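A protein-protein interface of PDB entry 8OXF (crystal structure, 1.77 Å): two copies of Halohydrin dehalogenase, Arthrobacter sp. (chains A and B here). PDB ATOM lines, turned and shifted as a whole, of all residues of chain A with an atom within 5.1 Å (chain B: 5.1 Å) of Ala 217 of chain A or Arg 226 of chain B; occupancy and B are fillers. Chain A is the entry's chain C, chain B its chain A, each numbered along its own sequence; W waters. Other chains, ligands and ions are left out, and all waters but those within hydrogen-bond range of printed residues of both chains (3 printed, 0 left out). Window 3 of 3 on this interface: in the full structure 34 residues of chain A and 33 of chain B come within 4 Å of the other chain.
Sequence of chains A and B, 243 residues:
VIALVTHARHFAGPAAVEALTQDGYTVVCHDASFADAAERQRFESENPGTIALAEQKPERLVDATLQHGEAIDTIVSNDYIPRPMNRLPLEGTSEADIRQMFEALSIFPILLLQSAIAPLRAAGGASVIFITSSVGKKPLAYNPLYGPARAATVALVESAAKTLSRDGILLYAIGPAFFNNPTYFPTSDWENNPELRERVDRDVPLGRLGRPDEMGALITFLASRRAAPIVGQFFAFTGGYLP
Ala 217 of chain A touches just these residues of chain B: Phe 221 and Arg 226. Of the printed residues of chain A, Arg 226 of chain B touches Glu 214 and Ala 217. Printed residues of chain A within 4 Å of Ala 228 of chain B: Glu 214 (3.6 Å). Printed residues of chain A within 4 Å of Phe 221 of chain B: Ala 217 (3.7 Å), Leu 218 (3.9 Å) and Phe 221 (3.5 Å). Printed residues of chain A within 4 Å of Ala 227 of chain B: Glu 214. Of the printed residues of chain B, Leu 218 of chain A touches Phe 221 (3.9 Å). Of the printed residues of chain B, Glu 214 of chain A touches Arg 226 (3.3 Å), Ala 227 (3.7 Å) and Ala 228 (3.6 Å). Ser 224 of chain B touches none of the printed residues of chain A. The nearest residue of chain B that does not touch Ala 217 of chain A is Ala 227 of chain B (4.6 Å). The nearest residue of chain A that does not touch Arg 226 of chain B is Thr 220 of chain A (4.2 Å). The nearest printed residue of chain B that does not touch Leu 218 of chain A is Ala 227 of chain B (4.2 Å).
Phe 221 of chain B touches its own counterpart, Phe 221 of chain A.
Printed residues of chain A that touch a printed residue of chain B: Glu 214, Ala 217, Leu 218 and Phe 221. Hydrophobic or aromatic side chains of chain A that line the printed part of chain B: Ala 217 and Phe 221. Printed residues of chain B that touch a printed residue of chain A: Phe 221, Arg 226, Ala 227 and Ala 228. Hydrophobic or aromatic side chains of chain B that line the printed part of chain A: Phe 221, Ala 227 and Ala 228. Among the printed residues, no Asp or Glu carboxylate lies within 4 Å of a Lys or Arg side-chain nitrogen of the other chain.
Among the printed residues, merely in contact across the chains: Glu 214 of chain A with Arg 226 of chain B, Phe 221 of chain A with Phe 221 of chain B, Glu 214 of chain A with Ala 228 of chain B, Ala 217 of chain A with Arg 226 of chain B, Ala 217 of chain A with Phe 221 of chain B, Glu 214 of chain A with Ala 227 of chain B and Leu 218 of chain A with Phe 221 of chain B.
The backbone NH (N) of Arg 226 of chain B sits close to the side-chain hydroxyl (OG) of Ser 224 of chain B (3.3 Å). The backbone carbonyl oxygen (O) of Phe 221 of chain B sits at hydrogen-bond distance from the side-chain hydroxyl (OG) of Ser 224 of chain B, at 2.6 Å.
Water W1 lies within hydrogen-bond range of NH1 of Arg 226 of chain B and O of Ala 217 of chain A. Water W2 lies within hydrogen-bond range of the backbone carbonyl oxygen of Arg 225 of chain B (2.6 Å) and the side-chain carboxylate of Glu 214 of chain A (2.6 Å). Water W3 lies within hydrogen-bond range of the side-chain carboxylate of Asp 213 of chain A and the backbone carbonyl oxygen of Arg 226 of chain B.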
ATOM      1  N   ALA A  19       4.013  11.282 -14.467  1.00  0.00           N
ATOM      2  CA  ALA A  19       2.713  11.544 -15.091  1.00  0.00           C
ATOM      3  C   ALA A  19       2.839  11.716 -16.598  1.00  0.00           C
ATOM      4  O   ALA A  19       2.014  11.195 -17.362  1.00  0.00           O
ATOM      5  CB  ALA A  19       2.071  12.779 -14.471  1.00  0.00           C
ATOM      6  N   PRO A 212       1.810  13.802  -5.218  1.00  0.00           N
ATOM      7  CA  PRO A 212       2.516  13.880  -6.512  1.00  0.00           C
ATOM      8  C   PRO A 212       1.632  13.594  -7.728  1.00  0.00           C
ATOM      9  O   PRO A 212       1.778  14.284  -8.749  1.00  0.00           O
ATOM     10  CB  PRO A 212       3.664  12.863  -6.348  1.00  0.00           C
ATOM     11  CG  PRO A 212       3.335  12.059  -5.140  1.00  0.00           C
ATOM     12  CD  PRO A 212       2.525  12.949  -4.250  1.00  0.00           C
ATOM     13  N   ASP A 213       0.700  12.629  -7.657  1.00  0.00           N
ATOM     14  CA  ASP A 213      -0.146  12.373  -8.817  1.00  0.00           C
ATOM     15  C   ASP A 213      -1.118  13.527  -9.081  1.00  0.00           C
ATOM     16  O   ASP A 213      -1.541  13.720 -10.224  1.00  0.00           O
ATOM     17  CB  ASP A 213      -0.905  11.050  -8.661  1.00  0.00           C
ATOM     18  CG  ASP A 213      -1.872  11.053  -7.491  1.00  0.00           C
ATOM     19  OD1 ASP A 213      -1.429  10.790  -6.358  1.00  0.00           O
ATOM     20  OD2 ASP A 213      -3.078  11.315  -7.701  1.00  0.00           O
ATOM     21  N   GLU A 214      -1.460  14.318  -8.058  1.00  0.00           N
ATOM     22  CA  GLU A 214      -2.316  15.486  -8.277  1.00  0.00           C
ATOM     23  C   GLU A 214      -1.558  16.607  -8.987  1.00  0.00           C
ATOM     24  O   GLU A 214      -2.107  17.265  -9.878  1.00  0.00           O
ATOM     25  CB  GLU A 214      -2.898  15.973  -6.940  1.00  0.00           C
ATOM     26  CG  GLU A 214      -3.753  14.916  -6.275  1.00  0.00           C
ATOM     27  CD  GLU A 214      -4.315  15.313  -4.916  1.00  0.00           C
ATOM     28  OE1 GLU A 214      -3.532  15.633  -3.986  1.00  0.00           O
ATOM     29  OE2 GLU A 214      -5.554  15.290  -4.777  1.00  0.00           O
ATOM     30  N   MET A 215      -0.289  16.829  -8.617  1.00  0.00           N
ATOM     31  CA  MET A 215       0.560  17.730  -9.394  1.00  0.00           C
ATOM     32  C   MET A 215       0.753  17.208 -10.803  1.00  0.00           C
ATOM     33  O   MET A 215       0.697  17.979 -11.767  1.00  0.00           O
ATOM     34  CB  MET A 215       1.916  17.925  -8.709  1.00  0.00           C
ATOM     35  CG  MET A 215       2.934  18.678  -9.575  1.00  0.00           C
ATOM     36  SD  MET A 215       2.552  20.461  -9.683  1.00  0.00           S
ATOM     37  CE  MET A 215       2.920  21.013  -8.009  1.00  0.00           C
ATOM     38  N   GLY A 216       0.935  15.890 -10.948  1.00  0.00           N
ATOM     39  CA  GLY A 216       1.088  15.313 -12.276  1.00  0.00           C
ATOM     40  C   GLY A 216      -0.171  15.438 -13.121  1.00  0.00           C
ATOM     41  O   GLY A 216      -0.096  15.631 -14.339  1.00  0.00           O
ATOM     42  N   ALA A 217      -1.343  15.316 -12.485  1.00  0.00           N
ATOM     43  CA  ALA A 217      -2.603  15.547 -13.188  1.00  0.00           C
ATOM     44  C   ALA A 217      -2.716  16.989 -13.665  1.00  0.00           C
ATOM     45  O   ALA A 217      -3.188  17.238 -14.777  1.00  0.00           O
ATOM     46  CB  ALA A 217      -3.798  15.194 -12.298  1.00  0.00           C
ATOM     47  N   LEU A 218      -2.326  17.960 -12.830  1.00  0.00           N
ATOM     48  CA  LEU A 218      -2.399  19.344 -13.281  1.00  0.00           C
ATOM     49  C   LEU A 218      -1.447  19.578 -14.453  1.00  0.00           C
ATOM     50  O   LEU A 218      -1.835  20.168 -15.469  1.00  0.00           O
ATOM     51  CB  LEU A 218      -2.108  20.299 -12.118  1.00  0.00           C
ATOM     52  CG  LEU A 218      -1.965  21.768 -12.500  1.00  0.00           C
ATOM     53  CD1 LEU A 218      -3.263  22.226 -13.170  1.00  0.00           C
ATOM     54  CD2 LEU A 218      -1.687  22.599 -11.261  1.00  0.00           C
ATOM     55  N   ILE A 219      -0.211  19.073 -14.348  1.00  0.00           N
ATOM     56  CA  ILE A 219       0.774  19.234 -15.418  1.00  0.00           C
ATOM     57  C   ILE A 219       0.263  18.604 -16.705  1.00  0.00           C
ATOM     58  O   ILE A 219       0.320  19.202 -17.791  1.00  0.00           O
ATOM     59  CB  ILE A 219       2.115  18.614 -14.990  1.00  0.00           C
ATOM     60  CG1 ILE A 219       2.752  19.445 -13.871  1.00  0.00           C
ATOM     61  CG2 ILE A 219       3.059  18.497 -16.183  1.00  0.00           C
ATOM     62  CD1 ILE A 219       4.073  18.865 -13.365  1.00  0.00           C
ATOM     63  N   THR A 220      -0.250  17.383 -16.596  1.00  0.00           N
ATOM     64  CA  THR A 220      -0.663  16.637 -17.773  1.00  0.00           C
ATOM     65  C   THR A 220      -1.894  17.285 -18.416  1.00  0.00           C
ATOM     66  O   THR A 220      -1.990  17.372 -19.647  1.00  0.00           O
ATOM     67  CB  THR A 220      -0.862  15.169 -17.346  1.00  0.00           C
ATOM     68  OG1 THR A 220      -0.116  14.298 -18.205  1.00  0.00           O
ATOM     69  CG2 THR A 220      -2.296  14.737 -17.253  1.00  0.00           C
ATOM     70  N   PHE A 221      -2.802  17.824 -17.595  1.00  0.00           N
ATOM     71  CA  PHE A 221      -3.952  18.561 -18.117  1.00  0.00           C
ATOM     72  C   PHE A 221      -3.506  19.810 -18.871  1.00  0.00           C
ATOM     73  O   PHE A 221      -3.991  20.089 -19.971  1.00  0.00           O
ATOM     74  CB  PHE A 221      -4.906  18.951 -16.981  1.00  0.00           C
ATOM     75  CG  PHE A 221      -6.061  19.821 -17.432  1.00  0.00           C
ATOM     76  CD1 PHE A 221      -7.021  19.316 -18.291  1.00  0.00           C
ATOM     77  CD2 PHE A 221      -6.162  21.150 -17.027  1.00  0.00           C
ATOM     78  CE1 PHE A 221      -8.082  20.116 -18.721  1.00  0.00           C
ATOM     79  CE2 PHE A 221      -7.222  21.958 -17.464  1.00  0.00           C
ATOM     80  CZ  PHE A 221      -8.175  21.434 -18.293  1.00  0.00           C
ATOM     81  N   LEU A 222      -2.592  20.590 -18.278  1.00  0.00           N
ATOM     82  CA  LEU A 222      -2.072  21.761 -18.978  1.00  0.00           C
ATOM     83  C   LEU A 222      -1.351  21.362 -20.259  1.00  0.00           C
ATOM     84  O   LEU A 222      -1.447  22.054 -21.275  1.00  0.00           O
ATOM     85  CB  LEU A 222      -1.137  22.570 -18.063  1.00  0.00           C
ATOM     86  CG  LEU A 222      -1.773  23.179 -16.800  1.00  0.00           C
ATOM     87  CD1 LEU A 222      -0.755  23.934 -15.937  1.00  0.00           C
ATOM     88  CD2 LEU A 222      -2.937  24.087 -17.154  1.00  0.00           C
ATOM     89  N   PHE B 221     -12.283  18.515 -15.996  1.00  0.00           N
ATOM     90  CA  PHE B 221     -11.062  18.381 -15.203  1.00  0.00           C
ATOM     91  C   PHE B 221     -11.308  18.728 -13.731  1.00  0.00           C
ATOM     92  O   PHE B 221     -10.845  18.022 -12.827  1.00  0.00           O
ATOM     93  CB  PHE B 221      -9.954  19.272 -15.788  1.00  0.00           C
ATOM     94  CG  PHE B 221      -8.674  19.272 -14.982  1.00  0.00           C
ATOM     95  CD1 PHE B 221      -7.893  18.118 -14.872  1.00  0.00           C
ATOM     96  CD2 PHE B 221      -8.254  20.427 -14.326  1.00  0.00           C
ATOM     97  CE1 PHE B 221      -6.714  18.128 -14.131  1.00  0.00           C
ATOM     98  CE2 PHE B 221      -7.071  20.444 -13.582  1.00  0.00           C
ATOM     99  CZ  PHE B 221      -6.306  19.293 -13.479  1.00  0.00           C
ATOM    100  N   SER B 224     -13.342  15.997 -11.993  1.00  0.00           N
ATOM    101  CA  SER B 224     -12.645  14.737 -11.783  1.00  0.00           C
ATOM    102  C   SER B 224     -12.004  14.643 -10.406  1.00  0.00           C
ATOM    103  O   SER B 224     -11.737  13.528  -9.949  1.00  0.00           O
ATOM    104  CB  SER B 224     -11.567  14.540 -12.865  1.00  0.00           C
ATOM    105  OG  SER B 224     -10.481  15.414 -12.632  1.00  0.00           O
ATOM    106  N   ARG B 225     -11.755  15.781  -9.736  1.00  0.00           N
ATOM    107  CA  ARG B 225     -11.069  15.881  -8.440  1.00  0.00           C
ATOM    108  C   ARG B 225      -9.612  15.444  -8.506  1.00  0.00           C
ATOM    109  O   ARG B 225      -8.968  15.278  -7.466  1.00  0.00           O
ATOM    110  CB  ARG B 225     -11.776  15.083  -7.343  1.00  0.00           C
ATOM    111  CG  ARG B 225     -13.206  15.510  -7.167  1.00  0.00           C
ATOM    112  CD  ARG B 225     -13.800  14.941  -5.884  1.00  0.00           C
ATOM    113  NE  ARG B 225     -15.167  14.499  -6.105  1.00  0.00           N
ATOM    114  CZ  ARG B 225     -15.908  13.883  -5.197  1.00  0.00           C
ATOM    115  NH1 ARG B 225     -15.441  13.624  -3.986  1.00  0.00           N
ATOM    116  NH2 ARG B 225     -17.145  13.504  -5.519  1.00  0.00           N
ATOM    117  N   ARG B 226      -9.068  15.279  -9.706  1.00  0.00           N
ATOM    118  CA  ARG B 226      -7.745  14.692  -9.848  1.00  0.00           C
ATOM    119  C   ARG B 226      -6.638  15.660  -9.435  1.00  0.00           C
ATOM    120  O   ARG B 226      -5.538  15.208  -9.089  1.00  0.00           O
ATOM    121  CB  ARG B 226      -7.578  14.222 -11.292  1.00  0.00           C
ATOM    122  CG  ARG B 226      -8.131  12.812 -11.527  1.00  0.00           C
ATOM    123  CD  ARG B 226      -8.089  12.471 -12.998  1.00  0.00           C
ATOM    124  NE  ARG B 226      -6.723  12.238 -13.450  1.00  0.00           N
ATOM    125  CZ  ARG B 226      -6.115  12.959 -14.385  1.00  0.00           C
ATOM    126  NH1 ARG B 226      -6.735  13.962 -14.991  1.00  0.00           N
ATOM    127  NH2 ARG B 226      -4.849  12.671 -14.711  1.00  0.00           N
ATOM    128  N   ALA B 227      -6.899  16.974  -9.451  1.00  0.00           N
ATOM    129  CA  ALA B 227      -5.930  17.950  -8.954  1.00  0.00           C
ATOM    130  C   ALA B 227      -6.528  18.773  -7.811  1.00  0.00           C
ATOM    131  O   ALA B 227      -6.388  19.999  -7.779  1.00  0.00           O
ATOM    132  CB  ALA B 227      -5.445  18.868 -10.088  1.00  0.00           C
ATOM    133  N   ALA B 228      -7.168  18.102  -6.848  1.00  0.00           N
ATOM    134  CA  ALA B 228      -7.837  18.723  -5.705  1.00  0.00           C
ATOM    135  C   ALA B 228      -7.039  19.829  -4.998  1.00  0.00           C
ATOM    136  O   ALA B 228      -7.652  20.793  -4.529  1.00  0.00           O
ATOM    137  CB  ALA B 228      -8.220  17.648  -4.686  1.00  0.00           C
HETATM  138  O   HOH W   1      -5.130  15.361 -16.200  1.00  0.00           O
HETATM  139  O   HOH W   2      -7.336  13.845  -6.048  1.00  0.00           O
HETATM  140  O   HOH W   3      -4.889  12.475  -9.372  1.00  0.00           O
